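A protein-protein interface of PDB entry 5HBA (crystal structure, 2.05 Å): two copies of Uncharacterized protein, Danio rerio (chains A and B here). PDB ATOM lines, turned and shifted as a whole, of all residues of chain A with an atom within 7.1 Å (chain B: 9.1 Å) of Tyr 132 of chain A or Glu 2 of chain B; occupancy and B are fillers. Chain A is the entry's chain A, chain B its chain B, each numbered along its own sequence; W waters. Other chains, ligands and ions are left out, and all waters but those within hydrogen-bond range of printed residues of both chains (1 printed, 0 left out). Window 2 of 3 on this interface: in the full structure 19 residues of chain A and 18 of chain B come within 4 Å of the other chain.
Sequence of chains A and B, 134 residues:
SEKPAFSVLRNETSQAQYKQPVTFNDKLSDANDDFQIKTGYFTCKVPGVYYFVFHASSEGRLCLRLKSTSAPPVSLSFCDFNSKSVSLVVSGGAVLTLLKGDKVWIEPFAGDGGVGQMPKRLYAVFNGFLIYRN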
ATOM      1  N   LYS A   3     -12.611  27.557 -28.176  1.00  0.00           N
ATOM      2  CA  LYS A   3     -12.221  27.029 -26.868  1.00  0.00           C
ATOM      3  C   LYS A   3     -12.801  27.920 -25.759  1.00  0.00           C
ATOM      4  O   LYS A   3     -13.390  28.964 -26.062  1.00  0.00           O
ATOM      5  CB  LYS A   3     -10.693  26.890 -26.765  1.00  0.00           C
ATOM      6  CG  LYS A   3      -9.895  28.149 -27.051  1.00  0.00           C
ATOM      7  CD  LYS A   3      -8.402  27.826 -27.024  1.00  0.00           C
ATOM      8  CE  LYS A   3      -7.570  28.982 -27.545  1.00  0.00           C
ATOM      9  NZ  LYS A   3      -6.120  28.664 -27.504  1.00  0.00           N
ATOM     10  N   VAL A  46     -13.285  21.758 -19.903  1.00  0.00           N
ATOM     11  CA  VAL A  46     -12.082  21.334 -20.619  1.00  0.00           C
ATOM     12  C   VAL A  46     -10.846  21.437 -19.729  1.00  0.00           C
ATOM     13  O   VAL A  46     -10.390  22.540 -19.417  1.00  0.00           O
ATOM     14  CB  VAL A  46     -11.848  22.216 -21.859  1.00  0.00           C
ATOM     15  CG1 VAL A  46     -10.569  21.799 -22.579  1.00  0.00           C
ATOM     16  CG2 VAL A  46     -13.043  22.152 -22.797  1.00  0.00           C
ATOM     17  N   PRO A  47     -10.288  20.287 -19.319  1.00  0.00           N
ATOM     18  CA  PRO A  47      -9.104  20.265 -18.450  1.00  0.00           C
ATOM     19  C   PRO A  47      -7.911  20.925 -19.130  1.00  0.00           C
ATOM     20  O   PRO A  47      -7.683  20.694 -20.319  1.00  0.00           O
ATOM     21  CB  PRO A  47      -8.829  18.765 -18.265  1.00  0.00           C
ATOM     22  CG  PRO A  47     -10.132  18.088 -18.617  1.00  0.00           C
ATOM     23  CD  PRO A  47     -10.727  18.932 -19.692  1.00  0.00           C
ATOM     24  N   GLY A  48      -7.158  21.738 -18.394  1.00  0.00           N
ATOM     25  CA  GLY A  48      -6.023  22.418 -18.990  1.00  0.00           C
ATOM     26  C   GLY A  48      -5.504  23.590 -18.179  1.00  0.00           C
ATOM     27  O   GLY A  48      -5.817  23.737 -16.992  1.00  0.00           O
ATOM     28  N   VAL A  49      -4.701  24.420 -18.834  1.00  0.00           N
ATOM     29  CA  VAL A  49      -4.090  25.571 -18.193  1.00  0.00           C
ATOM     30  C   VAL A  49      -4.827  26.826 -18.669  1.00  0.00           C
ATOM     31  O   VAL A  49      -5.041  27.013 -19.872  1.00  0.00           O
ATOM     32  CB  VAL A  49      -2.591  25.636 -18.518  1.00  0.00           C
ATOM     33  CG1 VAL A  49      -1.974  26.904 -17.962  1.00  0.00           C
ATOM     34  CG2 VAL A  49      -1.888  24.409 -17.939  1.00  0.00           C
ATOM     35  N   TYR A  50      -5.235  27.670 -17.722  1.00  0.00           N
ATOM     36  CA  TYR A  50      -6.105  28.800 -18.031  1.00  0.00           C
ATOM     37  C   TYR A  50      -5.498  30.117 -17.582  1.00  0.00           C
ATOM     38  O   TYR A  50      -4.699  30.141 -16.648  1.00  0.00           O
ATOM     39  CB  TYR A  50      -7.436  28.630 -17.297  1.00  0.00           C
ATOM     40  CG  TYR A  50      -8.377  27.627 -17.917  1.00  0.00           C
ATOM     41  CD1 TYR A  50      -8.215  26.264 -17.700  1.00  0.00           C
ATOM     42  CD2 TYR A  50      -9.443  28.050 -18.705  1.00  0.00           C
ATOM     43  CE1 TYR A  50      -9.088  25.344 -18.265  1.00  0.00           C
ATOM     44  CE2 TYR A  50     -10.319  27.146 -19.271  1.00  0.00           C
ATOM     45  CZ  TYR A  50     -10.135  25.793 -19.050  1.00  0.00           C
ATOM     46  OH  TYR A  50     -11.018  24.906 -19.619  1.00  0.00           O
ATOM     47  N   THR A  97      -3.818  25.786 -13.466  1.00  0.00           N
ATOM     48  CA  THR A  97      -4.074  24.467 -14.033  1.00  0.00           C
ATOM     49  C   THR A  97      -5.350  23.927 -13.412  1.00  0.00           C
ATOM     50  O   THR A  97      -5.446  23.836 -12.183  1.00  0.00           O
ATOM     51  CB  THR A  97      -2.928  23.484 -13.688  1.00  0.00           C
ATOM     52  OG1 THR A  97      -1.677  24.063 -14.062  1.00  0.00           O
ATOM     53  CG2 THR A  97      -3.112  22.168 -14.421  1.00  0.00           C
ATOM     54  N   PHE A 129      -9.673  32.594 -20.183  1.00  0.00           N
ATOM     55  CA  PHE A 129      -9.614  31.764 -21.385  1.00  0.00           C
ATOM     56  C   PHE A 129      -8.617  30.618 -21.252  1.00  0.00           C
ATOM     57  O   PHE A 129      -7.650  30.693 -20.481  1.00  0.00           O
ATOM     58  CB  PHE A 129      -9.332  32.605 -22.645  1.00  0.00           C
ATOM     59  CG  PHE A 129      -8.142  33.510 -22.521  1.00  0.00           C
ATOM     60  CD1 PHE A 129      -6.861  33.037 -22.790  1.00  0.00           C
ATOM     61  CD2 PHE A 129      -8.301  34.835 -22.142  1.00  0.00           C
ATOM     62  CE1 PHE A 129      -5.765  33.872 -22.679  1.00  0.00           C
ATOM     63  CE2 PHE A 129      -7.198  35.676 -22.024  1.00  0.00           C
ATOM     64  CZ  PHE A 129      -5.937  35.195 -22.299  1.00  0.00           C
ATOM     65  N   LEU A 130      -8.876  29.547 -21.996  1.00  0.00           N
ATOM     66  CA  LEU A 130      -7.973  28.405 -22.046  1.00  0.00           C
ATOM     67  C   LEU A 130      -6.681  28.793 -22.757  1.00  0.00           C
ATOM     68  O   LEU A 130      -6.716  29.435 -23.810  1.00  0.00           O
ATOM     69  CB  LEU A 130      -8.638  27.241 -22.796  1.00  0.00           C
ATOM     70  CG  LEU A 130      -7.750  26.006 -23.013  1.00  0.00           C
ATOM     71  CD1 LEU A 130      -7.561  25.285 -21.704  1.00  0.00           C
ATOM     72  CD2 LEU A 130      -8.320  25.064 -24.061  1.00  0.00           C
ATOM     73  N   ILE A 131      -5.544  28.409 -22.178  1.00  0.00           N
ATOM     74  CA  ILE A 131      -4.263  28.564 -22.861  1.00  0.00           C
ATOM     75  C   ILE A 131      -3.949  27.285 -23.646  1.00  0.00           C
ATOM     76  O   ILE A 131      -3.654  27.337 -24.842  1.00  0.00           O
ATOM     77  CB  ILE A 131      -3.122  28.903 -21.880  1.00  0.00           C
ATOM     78  CG1 ILE A 131      -3.396  30.248 -21.186  1.00  0.00           C
ATOM     79  CG2 ILE A 131      -1.780  28.933 -22.611  1.00  0.00           C
ATOM     80  CD1 ILE A 131      -2.524  30.477 -19.929  1.00  0.00           C
ATOM     81  N   TYR A 132      -4.011  26.138 -22.977  1.00  0.00           N
ATOM     82  CA  TYR A 132      -3.854  24.864 -23.679  1.00  0.00           C
ATOM     83  C   TYR A 132      -4.573  23.719 -22.970  1.00  0.00           C
ATOM     84  O   TYR A 132      -4.732  23.736 -21.742  1.00  0.00           O
ATOM     85  CB  TYR A 132      -2.368  24.545 -23.926  1.00  0.00           C
ATOM     86  CG  TYR A 132      -1.587  24.048 -22.721  1.00  0.00           C
ATOM     87  CD1 TYR A 132      -1.657  22.712 -22.325  1.00  0.00           C
ATOM     88  CD2 TYR A 132      -0.749  24.900 -22.004  1.00  0.00           C
ATOM     89  CE1 TYR A 132      -0.941  22.242 -21.235  1.00  0.00           C
ATOM     90  CE2 TYR A 132      -0.020  24.435 -20.908  1.00  0.00           C
ATOM     91  CZ  TYR A 132      -0.124  23.104 -20.533  1.00  0.00           C
ATOM     92  OH  TYR A 132       0.582  22.620 -19.450  1.00  0.00           O
ATOM     93  N   ARG A 133      -4.999  22.723 -23.746  1.00  0.00           N
ATOM     94  CA  ARG A 133      -5.703  21.556 -23.206  1.00  0.00           C
ATOM     95  C   ARG A 133      -4.769  20.561 -22.529  1.00  0.00           C
ATOM     96  O   ARG A 133      -3.735  20.198 -23.092  1.00  0.00           O
ATOM     97  CB  ARG A 133      -6.467  20.831 -24.320  1.00  0.00           C
ATOM     98  CG  ARG A 133      -7.727  21.524 -24.759  1.00  0.00           C
ATOM     99  CD  ARG A 133      -8.349  20.836 -25.965  1.00  0.00           C
ATOM    100  NE  ARG A 133      -9.682  21.367 -26.251  1.00  0.00           N
ATOM    101  CZ  ARG A 133      -9.922  22.451 -26.985  1.00  0.00           C
ATOM    102  NH1 ARG A 133      -8.917  23.134 -27.521  1.00  0.00           N
ATOM    103  NH2 ARG A 133     -11.169  22.854 -27.183  1.00  0.00           N
ATOM    104  N   ASN A 134      -5.151  20.118 -21.330  1.00  0.00           N
ATOM    105  CA  ASN A 134      -4.410  19.096 -20.580  1.00  0.00           C
ATOM    106  C   ASN A 134      -4.467  17.767 -21.315  1.00  0.00           C
ATOM    107  O   ASN A 134      -5.445  17.025 -21.179  1.00  0.00           O
ATOM    108  CB  ASN A 134      -5.015  18.891 -19.179  1.00  0.00           C
ATOM    109  CG  ASN A 134      -4.240  19.598 -18.081  1.00  0.00           C
ATOM    110  OD1 ASN A 134      -3.058  19.923 -18.241  1.00  0.00           O
ATOM    111  ND2 ASN A 134      -4.904  19.824 -16.939  1.00  0.00           N
ATOM    112  N   GLU B   2       1.304  21.117 -25.122  1.00  0.00           N
ATOM    113  CA  GLU B   2       1.531  21.990 -23.972  1.00  0.00           C
ATOM    114  C   GLU B   2       2.410  23.193 -24.332  1.00  0.00           C
ATOM    115  O   GLU B   2       3.382  23.057 -25.080  1.00  0.00           O
ATOM    116  CB  GLU B   2       2.152  21.205 -22.817  1.00  0.00           C
ATOM    117  N   LYS B   3       2.058  24.365 -23.799  1.00  0.00           N
ATOM    118  CA  LYS B   3       2.756  25.617 -24.105  1.00  0.00           C
ATOM    119  C   LYS B   3       3.493  26.150 -22.888  1.00  0.00           C
ATOM    120  O   LYS B   3       3.115  25.848 -21.756  1.00  0.00           O
ATOM    121  CB  LYS B   3       1.756  26.707 -24.505  1.00  0.00           C
ATOM    122  CG  LYS B   3       0.977  26.500 -25.782  1.00  0.00           C
ATOM    123  CD  LYS B   3      -0.123  27.553 -25.819  1.00  0.00           C
ATOM    124  CE  LYS B   3      -0.519  27.966 -27.218  1.00  0.00           C
ATOM    125  NZ  LYS B   3      -1.562  29.028 -27.136  1.00  0.00           N
ATOM    126  N   PRO B   4       4.533  26.968 -23.120  1.00  0.00           N
ATOM    127  CA  PRO B   4       5.074  27.767 -22.016  1.00  0.00           C
ATOM    128  C   PRO B   4       3.943  28.580 -21.393  1.00  0.00           C
ATOM    129  O   PRO B   4       3.203  29.265 -22.108  1.00  0.00           O
ATOM    130  CB  PRO B   4       6.061  28.705 -22.715  1.00  0.00           C
ATOM    131  CG  PRO B   4       6.525  27.926 -23.906  1.00  0.00           C
ATOM    132  CD  PRO B   4       5.306  27.140 -24.363  1.00  0.00           C
ATOM    133  N   ALA B   5       3.793  28.464 -20.078  1.00  0.00           N
ATOM    134  CA  ALA B   5       2.747  29.166 -19.345  1.00  0.00           C
ATOM    135  C   ALA B   5       3.110  29.102 -17.875  1.00  0.00           C
ATOM    136  O   ALA B   5       3.315  28.014 -17.331  1.00  0.00           O
ATOM    137  CB  ALA B   5       1.400  28.517 -19.583  1.00  0.00           C
ATOM    138  N   PHE B   6       3.208  30.257 -17.227  1.00  0.00           N
ATOM    139  CA  PHE B   6       3.622  30.261 -15.824  1.00  0.00           C
ATOM    140  C   PHE B   6       2.841  31.248 -14.967  1.00  0.00           C
ATOM    141  O   PHE B   6       2.268  32.230 -15.462  1.00  0.00           O
ATOM    142  CB  PHE B   6       5.131  30.528 -15.677  1.00  0.00           C
ATOM    143  CG  PHE B   6       5.527  31.957 -15.961  1.00  0.00           C
ATOM    144  CD1 PHE B   6       5.435  32.932 -14.973  1.00  0.00           C
ATOM    145  CD2 PHE B   6       6.007  32.319 -17.209  1.00  0.00           C
ATOM    146  CE1 PHE B   6       5.799  34.242 -15.226  1.00  0.00           C
ATOM    147  CE2 PHE B   6       6.377  33.629 -17.476  1.00  0.00           C
ATOM    148  CZ  PHE B   6       6.267  34.597 -16.483  1.00  0.00           C
ATOM    149  N   SER B  29       2.158  27.707 -11.385  1.00  0.00           N
ATOM    150  CA  SER B  29       2.153  27.018 -12.675  1.00  0.00           C
ATOM    151  C   SER B  29       3.456  27.308 -13.425  1.00  0.00           C
ATOM    152  O   SER B  29       3.983  28.419 -13.346  1.00  0.00           O
ATOM    153  CB  SER B  29       0.967  27.489 -13.522  1.00  0.00           C
ATOM    154  OG  SER B  29      -0.274  27.117 -12.937  1.00  0.00           O
ATOM    155  N   ASP B  30       3.974  26.312 -14.141  1.00  0.00           N
ATOM    156  CA  ASP B  30       5.108  26.504 -15.056  1.00  0.00           C
ATOM    157  C   ASP B  30       5.201  25.296 -15.991  1.00  0.00           C
ATOM    158  O   ASP B  30       6.003  24.386 -15.773  1.00  0.00           O
ATOM    159  CB  ASP B  30       6.422  26.697 -14.295  1.00  0.00           C
ATOM    160  CG  ASP B  30       7.580  27.081 -15.207  1.00  0.00           C
ATOM    161  OD1 ASP B  30       7.371  27.254 -16.436  1.00  0.00           O
ATOM    162  OD2 ASP B  30       8.705  27.222 -14.688  1.00  0.00           O
ATOM    163  N   ALA B  31       4.382  25.318 -17.039  1.00  0.00           N
ATOM    164  CA  ALA B  31       4.156  24.163 -17.910  1.00  0.00           C
ATOM    165  C   ALA B  31       5.383  23.638 -18.656  1.00  0.00           C
ATOM    166  O   ALA B  31       5.488  22.441 -18.912  1.00  0.00           O
ATOM    167  CB  ALA B  31       3.060  24.493 -18.903  1.00  0.00           C
ATOM    168  N   ASN B  32       6.290  24.537 -19.024  1.00  0.00           N
ATOM    169  CA  ASN B  32       7.453  24.184 -19.833  1.00  0.00           C
ATOM    170  C   ASN B  32       8.733  24.310 -19.012  1.00  0.00           C
ATOM    171  O   ASN B  32       9.836  24.237 -19.556  1.00  0.00           O
ATOM    172  CB  ASN B  32       7.508  25.103 -21.063  1.00  0.00           C
ATOM    173  CG  ASN B  32       8.492  24.627 -22.123  1.00  0.00           C
ATOM    174  OD1 ASN B  32       8.527  23.442 -22.473  1.00  0.00           O
ATOM    175  ND2 ASN B  32       9.300  25.557 -22.642  1.00  0.00           N
ATOM    176  N   ASP B  33       8.567  24.489 -17.699  1.00  0.00           N
ATOM    177  CA  ASP B  33       9.674  24.730 -16.762  1.00  0.00           C
ATOM    178  C   ASP B  33      10.596  25.869 -17.223  1.00  0.00           C
ATOM    179  O   ASP B  33      11.827  25.728 -17.251  1.00  0.00           O
ATOM    180  CB  ASP B  33      10.468  23.447 -16.484  1.00  0.00           C
ATOM    181  CG  ASP B  33      11.414  23.593 -15.302  1.00  0.00           C
ATOM    182  OD1 ASP B  33      11.118  24.411 -14.402  1.00  0.00           O
ATOM    183  OD2 ASP B  33      12.458  22.901 -15.273  1.00  0.00           O
ATOM    184  N   ASP B  34       9.985  26.995 -17.579  1.00  0.00           N
ATOM    185  CA  ASP B  34      10.707  28.146 -18.111  1.00  0.00           C
ATOM    186  C   ASP B  34      11.072  29.152 -17.030  1.00  0.00           C
ATOM    187  O   ASP B  34      11.920  30.019 -17.244  1.00  0.00           O
ATOM    188  CB  ASP B  34       9.852  28.874 -19.149  1.00  0.00           C
ATOM    189  CG  ASP B  34       9.703  28.107 -20.442  1.00  0.00           C
ATOM    190  OD1 ASP B  34      10.696  27.514 -20.913  1.00  0.00           O
ATOM    191  OD2 ASP B  34       8.595  28.119 -21.004  1.00  0.00           O
ATOM    192  N   VAL B  46      11.152  28.378 -26.145  1.00  0.00           N
ATOM    193  CA  VAL B  46      10.389  28.298 -27.385  1.00  0.00           C
ATOM    194  C   VAL B  46      10.189  29.691 -27.962  1.00  0.00           C
ATOM    195  O   VAL B  46       9.464  30.508 -27.391  1.00  0.00           O
ATOM    196  CB  VAL B  46       9.029  27.605 -27.172  1.00  0.00           C
ATOM    197  CG1 VAL B  46       8.198  27.658 -28.434  1.00  0.00           C
ATOM    198  CG2 VAL B  46       9.239  26.159 -26.735  1.00  0.00           C
ATOM    199  N   GLY B 128       2.781  34.610 -17.309  1.00  0.00           N
ATOM    200  CA  GLY B 128       3.169  34.713 -18.702  1.00  0.00           C
ATOM    201  C   GLY B 128       2.849  33.453 -19.482  1.00  0.00           C
ATOM    202  O   GLY B 128       2.808  32.362 -18.909  1.00  0.00           O
ATOM    203  N   PHE B 129       2.621  33.590 -20.783  1.00  0.00           N
ATOM    204  CA  PHE B 129       2.381  32.414 -21.620  1.00  0.00           C
ATOM    205  C   PHE B 129       2.652  32.688 -23.094  1.00  0.00           C
ATOM    206  O   PHE B 129       2.580  33.828 -23.560  1.00  0.00           O
ATOM    207  CB  PHE B 129       0.963  31.851 -21.421  1.00  0.00           C
ATOM    208  CG  PHE B 129      -0.128  32.877 -21.559  1.00  0.00           C
ATOM    209  CD1 PHE B 129      -0.668  33.177 -22.804  1.00  0.00           C
ATOM    210  CD2 PHE B 129      -0.627  33.534 -20.441  1.00  0.00           C
ATOM    211  CE1 PHE B 129      -1.674  34.123 -22.933  1.00  0.00           C
ATOM    212  CE2 PHE B 129      -1.645  34.478 -20.573  1.00  0.00           C
ATOM    213  CZ  PHE B 129      -2.160  34.769 -21.813  1.00  0.00           C
ATOM    214  N   LEU B 130       2.999  31.629 -23.814  1.00  0.00           N
ATOM    215  CA  LEU B 130       3.205  31.725 -25.246  1.00  0.00           C
ATOM    216  C   LEU B 130       1.860  32.003 -25.921  1.00  0.00           C
ATOM    217  O   LEU B 130       0.849  31.392 -25.578  1.00  0.00           O
ATOM    218  CB  LEU B 130       3.797  30.415 -25.771  1.00  0.00           C
ATOM    219  CG  LEU B 130       3.979  30.340 -27.287  1.00  0.00           C
ATOM    220  CD1 LEU B 130       5.272  31.021 -27.698  1.00  0.00           C
ATOM    221  CD2 LEU B 130       3.960  28.899 -27.749  1.00  0.00           C
ATOM    222  N   ARG B 133       3.983  30.251 -31.561  1.00  0.00           N
ATOM    223  CA  ARG B 133       5.358  29.873 -31.871  1.00  0.00           C
ATOM    224  C   ARG B 133       5.887  30.577 -33.115  1.00  0.00           C
ATOM    225  O   ARG B 133       5.167  30.745 -34.096  1.00  0.00           O
ATOM    226  CB  ARG B 133       5.454  28.357 -32.073  1.00  0.00           C
ATOM    227  CG  ARG B 133       5.263  27.550 -30.802  1.00  0.00           C
ATOM    228  CD  ARG B 133       4.917  26.095 -31.094  1.00  0.00           C
ATOM    229  NE  ARG B 133       4.402  25.413 -29.908  1.00  0.00           N
ATOM    230  CZ  ARG B 133       3.145  25.501 -29.474  1.00  0.00           C
ATOM    231  NH1 ARG B 133       2.264  26.254 -30.124  1.00  0.00           N
ATOM    232  NH2 ARG B 133       2.765  24.840 -28.386  1.00  0.00           N
HETATM  233  O   HOH W   1      -2.102  26.079 -10.640  1.00  0.00           O
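The backbone carbonyl oxygen (O) of Val 49 of chain A sits at hydrogen-bond distance from the backbone NH (N) of Ile 131 of chain A (2.7 Å).
The backbone NH of Val 49 of chain A sits at hydrogen-bond distance from the backbone carbonyl oxygen of Tyr 132 of chain A (3.0 Å).
O of Ala 5 of chain B sits at hydrogen-bond distance from N of Ala 31 of chain B (2.9 Å).
OG of Ser 29 of chain B touches OG1 of Thr 97 of chain A (3.5 Å).
Phe 129 of chain B touches Phe 129 of chain A.
Lys 3 of chain B touches Ile 131 of chain A (NZ to O, 3.5 Å).
CD2 of Phe 129 of chain B touches CD1 of Ile 131 of chain A, at 3.6 Å.
CE1 of Tyr 132 of chain A touches CB of Glu 2 of chain B (3.6 Å).
Lys 3 of chain B touches Tyr 132 of chain A.
CB of Ala 31 of chain B touches OH of Tyr 132 of chain A, 3.2 Å away.
Tyr 132 of chain A touches three residues of chain B.
Glu 2 of chain B touches just one residue of chain A: Tyr 132.
No residue of chain B comes within 4 Å of Gly 48 of chain A.
No residue of chain B comes within 4 Å of Val 49 of chain A.
Of the printed residues of chain A, Ala 31 of chain B touches Tyr 132.
Of the printed residues of chain A, Ser 29 of chain B touches Thr 97.
Pro 4 of chain B touches none of the printed residues of chain A.
Leu 130 of chain A touches none of the printed residues of chain B.
The nearest residue of chain A that does not touch Glu 2 of chain B is Arg 133 of chain A (5.5 Å).
The nearest printed residue of chain B that does not touch Ile 131 of chain A is Ala 5 of chain B (4.4 Å).
Hydrophobic or aromatic side chains of chain B that line the printed part of chain A: Ala 31 and Phe 129.
Hydrophobic or aromatic side chains of chain A that line the printed part of chain B: Phe 129, Ile 131 and Tyr 132.
Among the printed residues, no Asp or Glu carboxylate lies within 4 Å of a Lys or Arg side-chain nitrogen of the other chain.
Phe 129 of chain B touches its own counterpart, Phe 129 of chain A.
5 positions are printed for both chains.
Of the 7 pairs that touch across the chains among the printed residues, 1 has its exchanged pair printed and touching as well.
Water W1 lies within hydrogen-bond range of the side-chain hydroxyl of Ser 29 of chain B (3.1 Å) and the backbone NH of Thr 97 of chain A (3.3 Å).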
